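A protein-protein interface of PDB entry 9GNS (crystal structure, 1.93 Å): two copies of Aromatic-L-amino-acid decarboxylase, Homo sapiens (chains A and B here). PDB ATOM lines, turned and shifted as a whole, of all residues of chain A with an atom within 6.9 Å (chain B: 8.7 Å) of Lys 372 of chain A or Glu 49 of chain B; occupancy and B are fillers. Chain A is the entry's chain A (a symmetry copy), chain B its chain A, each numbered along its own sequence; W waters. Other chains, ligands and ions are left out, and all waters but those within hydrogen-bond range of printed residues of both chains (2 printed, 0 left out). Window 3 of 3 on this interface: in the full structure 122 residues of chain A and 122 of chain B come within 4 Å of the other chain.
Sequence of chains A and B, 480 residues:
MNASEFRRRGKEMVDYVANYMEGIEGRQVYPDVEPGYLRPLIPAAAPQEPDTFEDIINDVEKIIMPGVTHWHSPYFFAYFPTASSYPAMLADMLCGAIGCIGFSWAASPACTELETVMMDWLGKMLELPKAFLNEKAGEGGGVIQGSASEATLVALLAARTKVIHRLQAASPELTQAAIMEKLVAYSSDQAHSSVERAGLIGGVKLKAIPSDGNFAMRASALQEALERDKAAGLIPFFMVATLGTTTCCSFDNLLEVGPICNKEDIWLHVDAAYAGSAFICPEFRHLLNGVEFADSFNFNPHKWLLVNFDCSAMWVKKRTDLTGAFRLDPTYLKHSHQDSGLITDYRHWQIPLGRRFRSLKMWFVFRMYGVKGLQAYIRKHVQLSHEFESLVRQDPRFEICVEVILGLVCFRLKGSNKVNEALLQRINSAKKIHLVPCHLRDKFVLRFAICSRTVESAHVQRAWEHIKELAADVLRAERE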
ATOM      1  N   ILE A 280      16.542   0.870  31.731  1.00  0.00           N
ATOM      2  CA  ILE A 280      17.661   1.211  30.853  1.00  0.00           C
ATOM      3  C   ILE A 280      17.203   1.565  29.448  1.00  0.00           C
ATOM      4  O   ILE A 280      18.008   2.060  28.646  1.00  0.00           O
ATOM      5  CB  ILE A 280      18.691   0.065  30.781  1.00  0.00           C
ATOM      6  CG1 ILE A 280      18.132  -1.112  29.977  1.00  0.00           C
ATOM      7  CG2 ILE A 280      19.109  -0.366  32.180  1.00  0.00           C
ATOM      8  CD1 ILE A 280      19.173  -2.165  29.650  1.00  0.00           C
ATOM      9  N   PHE A 366      27.785  -6.580  31.460  1.00  0.00           N
ATOM     10  CA  PHE A 366      27.726  -5.252  30.857  1.00  0.00           C
ATOM     11  C   PHE A 366      28.696  -5.129  29.691  1.00  0.00           C
ATOM     12  O   PHE A 366      28.361  -4.546  28.653  1.00  0.00           O
ATOM     13  CB  PHE A 366      28.023  -4.172  31.904  1.00  0.00           C
ATOM     14  CG  PHE A 366      27.009  -4.102  33.018  1.00  0.00           C
ATOM     15  CD1 PHE A 366      25.771  -4.712  32.894  1.00  0.00           C
ATOM     16  CD2 PHE A 366      27.303  -3.430  34.192  1.00  0.00           C
ATOM     17  CE1 PHE A 366      24.842  -4.648  33.921  1.00  0.00           C
ATOM     18  CE2 PHE A 366      26.381  -3.358  35.220  1.00  0.00           C
ATOM     19  CZ  PHE A 366      25.152  -3.970  35.088  1.00  0.00           C
ATOM     20  N   ARG A 367      29.907  -5.670  29.838  1.00  0.00           N
ATOM     21  CA  ARG A 367      30.889  -5.525  28.772  1.00  0.00           C
ATOM     22  C   ARG A 367      30.627  -6.474  27.613  1.00  0.00           C
ATOM     23  O   ARG A 367      30.893  -6.118  26.462  1.00  0.00           O
ATOM     24  CB  ARG A 367      32.305  -5.744  29.313  1.00  0.00           C
ATOM     25  CG  ARG A 367      32.737  -4.658  30.293  1.00  0.00           C
ATOM     26  CD  ARG A 367      34.183  -4.843  30.734  1.00  0.00           C
ATOM     27  NE  ARG A 367      35.125  -4.604  29.646  1.00  0.00           N
ATOM     28  CZ  ARG A 367      36.440  -4.731  29.759  1.00  0.00           C
ATOM     29  NH1 ARG A 367      36.999  -5.133  30.888  1.00  0.00           N
ATOM     30  NH2 ARG A 367      37.216  -4.443  28.714  1.00  0.00           N
ATOM     31  N   MET A 368      30.114  -7.672  27.874  1.00  0.00           N
ATOM     32  CA  MET A 368      30.016  -8.616  26.777  1.00  0.00           C
ATOM     33  C   MET A 368      28.729  -8.431  25.986  1.00  0.00           C
ATOM     34  O   MET A 368      28.676  -8.803  24.808  1.00  0.00           O
ATOM     35  CB  MET A 368      30.087 -10.048  27.291  1.00  0.00           C
ATOM     36  CG  MET A 368      31.510 -10.376  27.668  1.00  0.00           C
ATOM     37  SD  MET A 368      31.852 -12.081  28.061  1.00  0.00           S
ATOM     38  CE  MET A 368      32.493 -12.461  26.424  1.00  0.00           C
ATOM     39  N   TYR A 369      27.688  -7.890  26.614  1.00  0.00           N
ATOM     40  CA  TYR A 369      26.468  -7.546  25.896  1.00  0.00           C
ATOM     41  C   TYR A 369      26.505  -6.124  25.365  1.00  0.00           C
ATOM     42  O   TYR A 369      25.995  -5.864  24.270  1.00  0.00           O
ATOM     43  CB  TYR A 369      25.250  -7.729  26.812  1.00  0.00           C
ATOM     44  CG  TYR A 369      24.737  -9.155  26.810  1.00  0.00           C
ATOM     45  CD1 TYR A 369      23.885  -9.610  25.805  1.00  0.00           C
ATOM     46  CD2 TYR A 369      25.147 -10.059  27.783  1.00  0.00           C
ATOM     47  CE1 TYR A 369      23.437 -10.929  25.789  1.00  0.00           C
ATOM     48  CE2 TYR A 369      24.705 -11.372  27.775  1.00  0.00           C
ATOM     49  CZ  TYR A 369      23.853 -11.803  26.776  1.00  0.00           C
ATOM     50  OH  TYR A 369      23.418 -13.113  26.771  1.00  0.00           O
ATOM     51  N   GLY A 370      27.114  -5.203  26.112  1.00  0.00           N
ATOM     52  CA  GLY A 370      26.986  -3.791  25.819  1.00  0.00           C
ATOM     53  C   GLY A 370      25.619  -3.284  26.229  1.00  0.00           C
ATOM     54  O   GLY A 370      24.686  -4.078  26.397  1.00  0.00           O
ATOM     55  N   VAL A 371      25.477  -1.968  26.405  1.00  0.00           N
ATOM     56  CA  VAL A 371      24.175  -1.426  26.794  1.00  0.00           C
ATOM     57  C   VAL A 371      23.133  -1.728  25.723  1.00  0.00           C
ATOM     58  O   VAL A 371      21.986  -2.074  26.030  1.00  0.00           O
ATOM     59  CB  VAL A 371      24.278   0.086  27.074  1.00  0.00           C
ATOM     60  CG1 VAL A 371      22.899   0.662  27.374  1.00  0.00           C
ATOM     61  CG2 VAL A 371      25.229   0.353  28.243  1.00  0.00           C
ATOM     62  N   LYS A 372      23.516  -1.626  24.450  1.00  0.00           N
ATOM     63  CA  LYS A 372      22.555  -1.882  23.379  1.00  0.00           C
ATOM     64  C   LYS A 372      22.115  -3.340  23.345  1.00  0.00           C
ATOM     65  O   LYS A 372      20.958  -3.626  23.012  1.00  0.00           O
ATOM     66  CB  LYS A 372      23.147  -1.461  22.035  1.00  0.00           C
ATOM     67  CG  LYS A 372      23.251   0.057  21.895  1.00  0.00           C
ATOM     68  CD  LYS A 372      23.879   0.471  20.575  1.00  0.00           C
ATOM     69  CE  LYS A 372      24.102   1.976  20.533  1.00  0.00           C
ATOM     70  NZ  LYS A 372      25.204   2.345  19.600  1.00  0.00           N
ATOM     71  N   GLY A 373      23.008  -4.270  23.690  1.00  0.00           N
ATOM     72  CA  GLY A 373      22.611  -5.666  23.753  1.00  0.00           C
ATOM     73  C   GLY A 373      21.612  -5.930  24.862  1.00  0.00           C
ATOM     74  O   GLY A 373      20.685  -6.732  24.702  1.00  0.00           O
ATOM     75  N   LEU A 374      21.780  -5.262  26.004  1.00  0.00           N
ATOM     76  CA  LEU A 374      20.811  -5.431  27.085  1.00  0.00           C
ATOM     77  C   LEU A 374      19.482  -4.776  26.731  1.00  0.00           C
ATOM     78  O   LEU A 374      18.411  -5.310  27.052  1.00  0.00           O
ATOM     79  CB  LEU A 374      21.369  -4.851  28.384  1.00  0.00           C
ATOM     80  CG  LEU A 374      22.618  -5.577  28.894  1.00  0.00           C
ATOM     81  CD1 LEU A 374      23.228  -4.827  30.066  1.00  0.00           C
ATOM     82  CD2 LEU A 374      22.303  -7.024  29.264  1.00  0.00           C
ATOM     83  N   GLN A 375      19.526  -3.617  26.076  1.00  0.00           N
ATOM     84  CA  GLN A 375      18.286  -2.973  25.651  1.00  0.00           C
ATOM     85  C   GLN A 375      17.527  -3.844  24.659  1.00  0.00           C
ATOM     86  O   GLN A 375      16.293  -3.939  24.721  1.00  0.00           O
ATOM     87  CB  GLN A 375      18.580  -1.605  25.041  1.00  0.00           C
ATOM     88  CG  GLN A 375      19.006  -0.559  26.053  1.00  0.00           C
ATOM     89  CD  GLN A 375      19.462   0.722  25.392  1.00  0.00           C
ATOM     90  OE1 GLN A 375      20.186   0.703  24.390  1.00  0.00           O
ATOM     91  NE2 GLN A 375      19.021   1.850  25.938  1.00  0.00           N
ATOM     92  N   ALA A 376      18.245  -4.487  23.735  1.00  0.00           N
ATOM     93  CA  ALA A 376      17.579  -5.353  22.767  1.00  0.00           C
ATOM     94  C   ALA A 376      16.932  -6.542  23.461  1.00  0.00           C
ATOM     95  O   ALA A 376      15.831  -6.971  23.087  1.00  0.00           O
ATOM     96  CB  ALA A 376      18.576  -5.822  21.708  1.00  0.00           C
ATOM     97  N   TYR A 377      17.602  -7.074  24.484  1.00  0.00           N
ATOM     98  CA  TYR A 377      17.073  -8.205  25.238  1.00  0.00           C
ATOM     99  C   TYR A 377      15.777  -7.829  25.952  1.00  0.00           C
ATOM    100  O   TYR A 377      14.788  -8.572  25.907  1.00  0.00           O
ATOM    101  CB  TYR A 377      18.143  -8.683  26.229  1.00  0.00           C
ATOM    102  CG  TYR A 377      17.630  -9.471  27.419  1.00  0.00           C
ATOM    103  CD1 TYR A 377      17.363 -10.830  27.318  1.00  0.00           C
ATOM    104  CD2 TYR A 377      17.439  -8.856  28.650  1.00  0.00           C
ATOM    105  CE1 TYR A 377      16.906 -11.550  28.412  1.00  0.00           C
ATOM    106  CE2 TYR A 377      16.982  -9.565  29.742  1.00  0.00           C
ATOM    107  CZ  TYR A 377      16.718 -10.913  29.617  1.00  0.00           C
ATOM    108  OH  TYR A 377      16.264 -11.625  30.708  1.00  0.00           O
ATOM    109  N   ARG A 379      13.729  -5.340  25.136  1.00  0.00           N
ATOM    110  CA  ARG A 379      12.685  -4.999  24.178  1.00  0.00           C
ATOM    111  C   ARG A 379      12.102  -6.229  23.501  1.00  0.00           C
ATOM    112  O   ARG A 379      10.905  -6.248  23.186  1.00  0.00           O
ATOM    113  CB  ARG A 379      13.223  -4.025  23.135  1.00  0.00           C
ATOM    114  CG  ARG A 379      13.394  -2.620  23.686  1.00  0.00           C
ATOM    115  CD  ARG A 379      14.377  -1.819  22.880  1.00  0.00           C
ATOM    116  NE  ARG A 379      14.432  -0.445  23.365  1.00  0.00           N
ATOM    117  CZ  ARG A 379      15.396   0.410  23.064  1.00  0.00           C
ATOM    118  NH1 ARG A 379      16.416   0.057  22.296  1.00  0.00           N
ATOM    119  NH2 ARG A 379      15.334   1.649  23.542  1.00  0.00           N
ATOM    120  N   ALA B  45      31.543   4.753  32.069  1.00  0.00           N
ATOM    121  CA  ALA B  45      30.225   4.237  31.721  1.00  0.00           C
ATOM    122  C   ALA B  45      30.377   2.895  31.024  1.00  0.00           C
ATOM    123  O   ALA B  45      31.429   2.578  30.463  1.00  0.00           O
ATOM    124  CB  ALA B  45      29.450   5.217  30.830  1.00  0.00           C
ATOM    125  N   ALA B  46      29.308   2.104  31.071  1.00  0.00           N
ATOM    126  CA  ALA B  46      29.297   0.825  30.379  1.00  0.00           C
ATOM    127  C   ALA B  46      29.453   1.046  28.875  1.00  0.00           C
ATOM    128  O   ALA B  46      29.037   2.080  28.347  1.00  0.00           O
ATOM    129  CB  ALA B  46      27.997   0.074  30.668  1.00  0.00           C
ATOM    130  N   PRO B  47      30.050   0.096  28.157  1.00  0.00           N
ATOM    131  CA  PRO B  47      30.185   0.265  26.704  1.00  0.00           C
ATOM    132  C   PRO B  47      28.844   0.069  26.017  1.00  0.00           C
ATOM    133  O   PRO B  47      28.032  -0.765  26.427  1.00  0.00           O
ATOM    134  CB  PRO B  47      31.180  -0.830  26.311  1.00  0.00           C
ATOM    135  CG  PRO B  47      30.938  -1.902  27.331  1.00  0.00           C
ATOM    136  CD  PRO B  47      30.626  -1.179  28.620  1.00  0.00           C
ATOM    137  N   GLN B  48      28.608   0.856  24.966  1.00  0.00           N
ATOM    138  CA  GLN B  48      27.365   0.702  24.221  1.00  0.00           C
ATOM    139  C   GLN B  48      27.389  -0.558  23.369  1.00  0.00           C
ATOM    140  O   GLN B  48      26.395  -1.288  23.303  1.00  0.00           O
ATOM    141  CB  GLN B  48      27.106   1.946  23.372  1.00  0.00           C
ATOM    142  CG  GLN B  48      26.733   3.142  24.228  1.00  0.00           C
ATOM    143  CD  GLN B  48      25.277   3.105  24.664  1.00  0.00           C
ATOM    144  OE1 GLN B  48      24.395   2.748  23.887  1.00  0.00           O
ATOM    145  NE2 GLN B  48      25.026   3.436  25.924  1.00  0.00           N
ATOM    146  N   GLU B  49      28.501  -0.834  22.738  1.00  0.00           N
ATOM    147  CA  GLU B  49      28.722  -2.032  21.950  1.00  0.00           C
ATOM    148  C   GLU B  49      29.569  -3.018  22.749  1.00  0.00           C
ATOM    149  O   GLU B  49      30.333  -2.608  23.625  1.00  0.00           O
ATOM    150  CB  GLU B  49      29.440  -1.682  20.642  1.00  0.00           C
ATOM    151  CG  GLU B  49      28.684  -0.700  19.756  1.00  0.00           C
ATOM    152  CD  GLU B  49      27.391  -1.258  19.194  1.00  0.00           C
ATOM    153  OE1 GLU B  49      27.189  -2.489  19.246  1.00  0.00           O
ATOM    154  OE2 GLU B  49      26.565  -0.455  18.706  1.00  0.00           O
ATOM    155  N   PRO B  50      29.471  -4.320  22.473  1.00  0.00           N
ATOM    156  CA  PRO B  50      30.202  -5.303  23.284  1.00  0.00           C
ATOM    157  C   PRO B  50      31.713  -5.144  23.168  1.00  0.00           C
ATOM    158  O   PRO B  50      32.242  -4.823  22.102  1.00  0.00           O
ATOM    159  CB  PRO B  50      29.747  -6.649  22.702  1.00  0.00           C
ATOM    160  CG  PRO B  50      28.506  -6.354  21.928  1.00  0.00           C
ATOM    161  CD  PRO B  50      28.682  -4.966  21.409  1.00  0.00           C
ATOM    162  N   ASP B  51      32.402  -5.377  24.282  1.00  0.00           N
ATOM    163  CA  ASP B  51      33.844  -5.583  24.305  1.00  0.00           C
ATOM    164  C   ASP B  51      34.157  -7.048  24.004  1.00  0.00           C
ATOM    165  O   ASP B  51      33.303  -7.926  24.139  1.00  0.00           O
ATOM    166  CB  ASP B  51      34.423  -5.210  25.674  1.00  0.00           C
ATOM    167  CG  ASP B  51      34.340  -3.720  25.972  1.00  0.00           C
ATOM    168  OD1 ASP B  51      34.279  -2.924  25.016  1.00  0.00           O
ATOM    169  OD2 ASP B  51      34.339  -3.345  27.170  1.00  0.00           O
ATOM    170  N   THR B  52      35.405  -7.314  23.624  1.00  0.00           N
ATOM    171  CA  THR B  52      35.815  -8.690  23.364  1.00  0.00           C
ATOM    172  C   THR B  52      36.179  -9.412  24.657  1.00  0.00           C
ATOM    173  O   THR B  52      36.599  -8.795  25.643  1.00  0.00           O
ATOM    174  CB  THR B  52      37.019  -8.742  22.427  1.00  0.00           C
ATOM    175  OG1 THR B  52      38.179  -8.295  23.137  1.00  0.00           O
ATOM    176  CG2 THR B  52      36.799  -7.859  21.200  1.00  0.00           C
HETATM  177  O   HOH W   1      21.673   2.730  23.831  1.00  0.00           O
HETATM  178  O   HOH W   2      34.524  -1.338  29.247  1.00  0.00           O
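Of the 8 printed residues of chain B, 6 touch a printed residue of chain A. Hydrophobic or aromatic side chains of chain A that line the printed part of chain B: Val 371. Among the printed residues, 13 pairs touch across the chains. Among the printed residues, Asp or Glu carboxylates within 4 Å of a Lys or Arg side-chain nitrogen of the other chain: Arg 367 of chain A with Asp 51 of chain B (2.9 Å) and Lys 372 of chain A with Glu 49 of chain B (3.2 Å).
Water W1 lies within hydrogen-bond range of OE1 of Gln 375 of chain A and OE1 of Gln 48 of chain B. Water W2 lies within hydrogen-bond range of OD2 of Asp 51 of chain B and NE of Arg 367 of chain A.
Among the printed residues, pairs that only touch across the chains: Met 368 of chain A with Pro 50 of chain B (3.2 Å), Gly 370 of chain A with Pro 47 of chain B (3.3 Å), Arg 367 of chain A with Pro 50 of chain B (3.4 Å), Tyr 369 of chain A with Pro 50 of chain B (3.5 Å), Gly 370 of chain A with Gln 48 of chain B (3.6 Å), Val 371 of chain A with Ala 46 of chain B (3.7 Å), Arg 367 of chain A with Pro 47 of chain B (3.9 Å) and Phe 366 of chain A with Pro 47 of chain B (3.9 Å).
Ile 280 of chain A touches none of the printed residues of chain B. Of the printed residues of chain B, Phe 366 of chain A touches Pro 47 (3.9 Å). Of chain B, only Ala 46 (3.7 Å), Pro 47 (2.8 Å) and Gln 48 (3.3 Å) come within 4 Å of Val 371 of chain A. Printed residues of chain B within 4 Å of Lys 372 of chain A: Gln 48 and Glu 49. Tyr 377 of chain A touches none of the printed residues of chain B. Of the printed residues of chain A, Pro 47 of chain B touches Phe 366 (3.9 Å), Arg 367 (3.9 Å), Gly 370 (3.3 Å) and Val 371 (2.8 Å). The nearest printed residue of chain B that does not touch Tyr 369 of chain A is Gln 48 of chain B (4.7 Å).
No position is printed for both chains.
The backbone carbonyl oxygen of Pro 47 of chain B is in hydrogen-bond range of the backbone NH of Val 371 of chain A (2.8 Å). The backbone carbonyl oxygen (O) of Gln 48 of chain B lies within hydrogen-bond range of the backbone NH (N) of Val 371 of chain A (3.3 Å). The backbone NH (N) of Lys 372 of chain A is in hydrogen-bond range of the backbone carbonyl oxygen (O) of Gln 48 of chain B, 3.1 Å away. The side-chain amino group (NZ) of Lys 372 of chain A lies within salt-bridge range of the side-chain carboxylate (OE2) of Glu 49 of chain B (3.2 Å). The guanidinium group of Arg 367 of chain A lies within salt-bridge range of the side-chain carboxylate of Asp 51 of chain B (2.9 Å).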
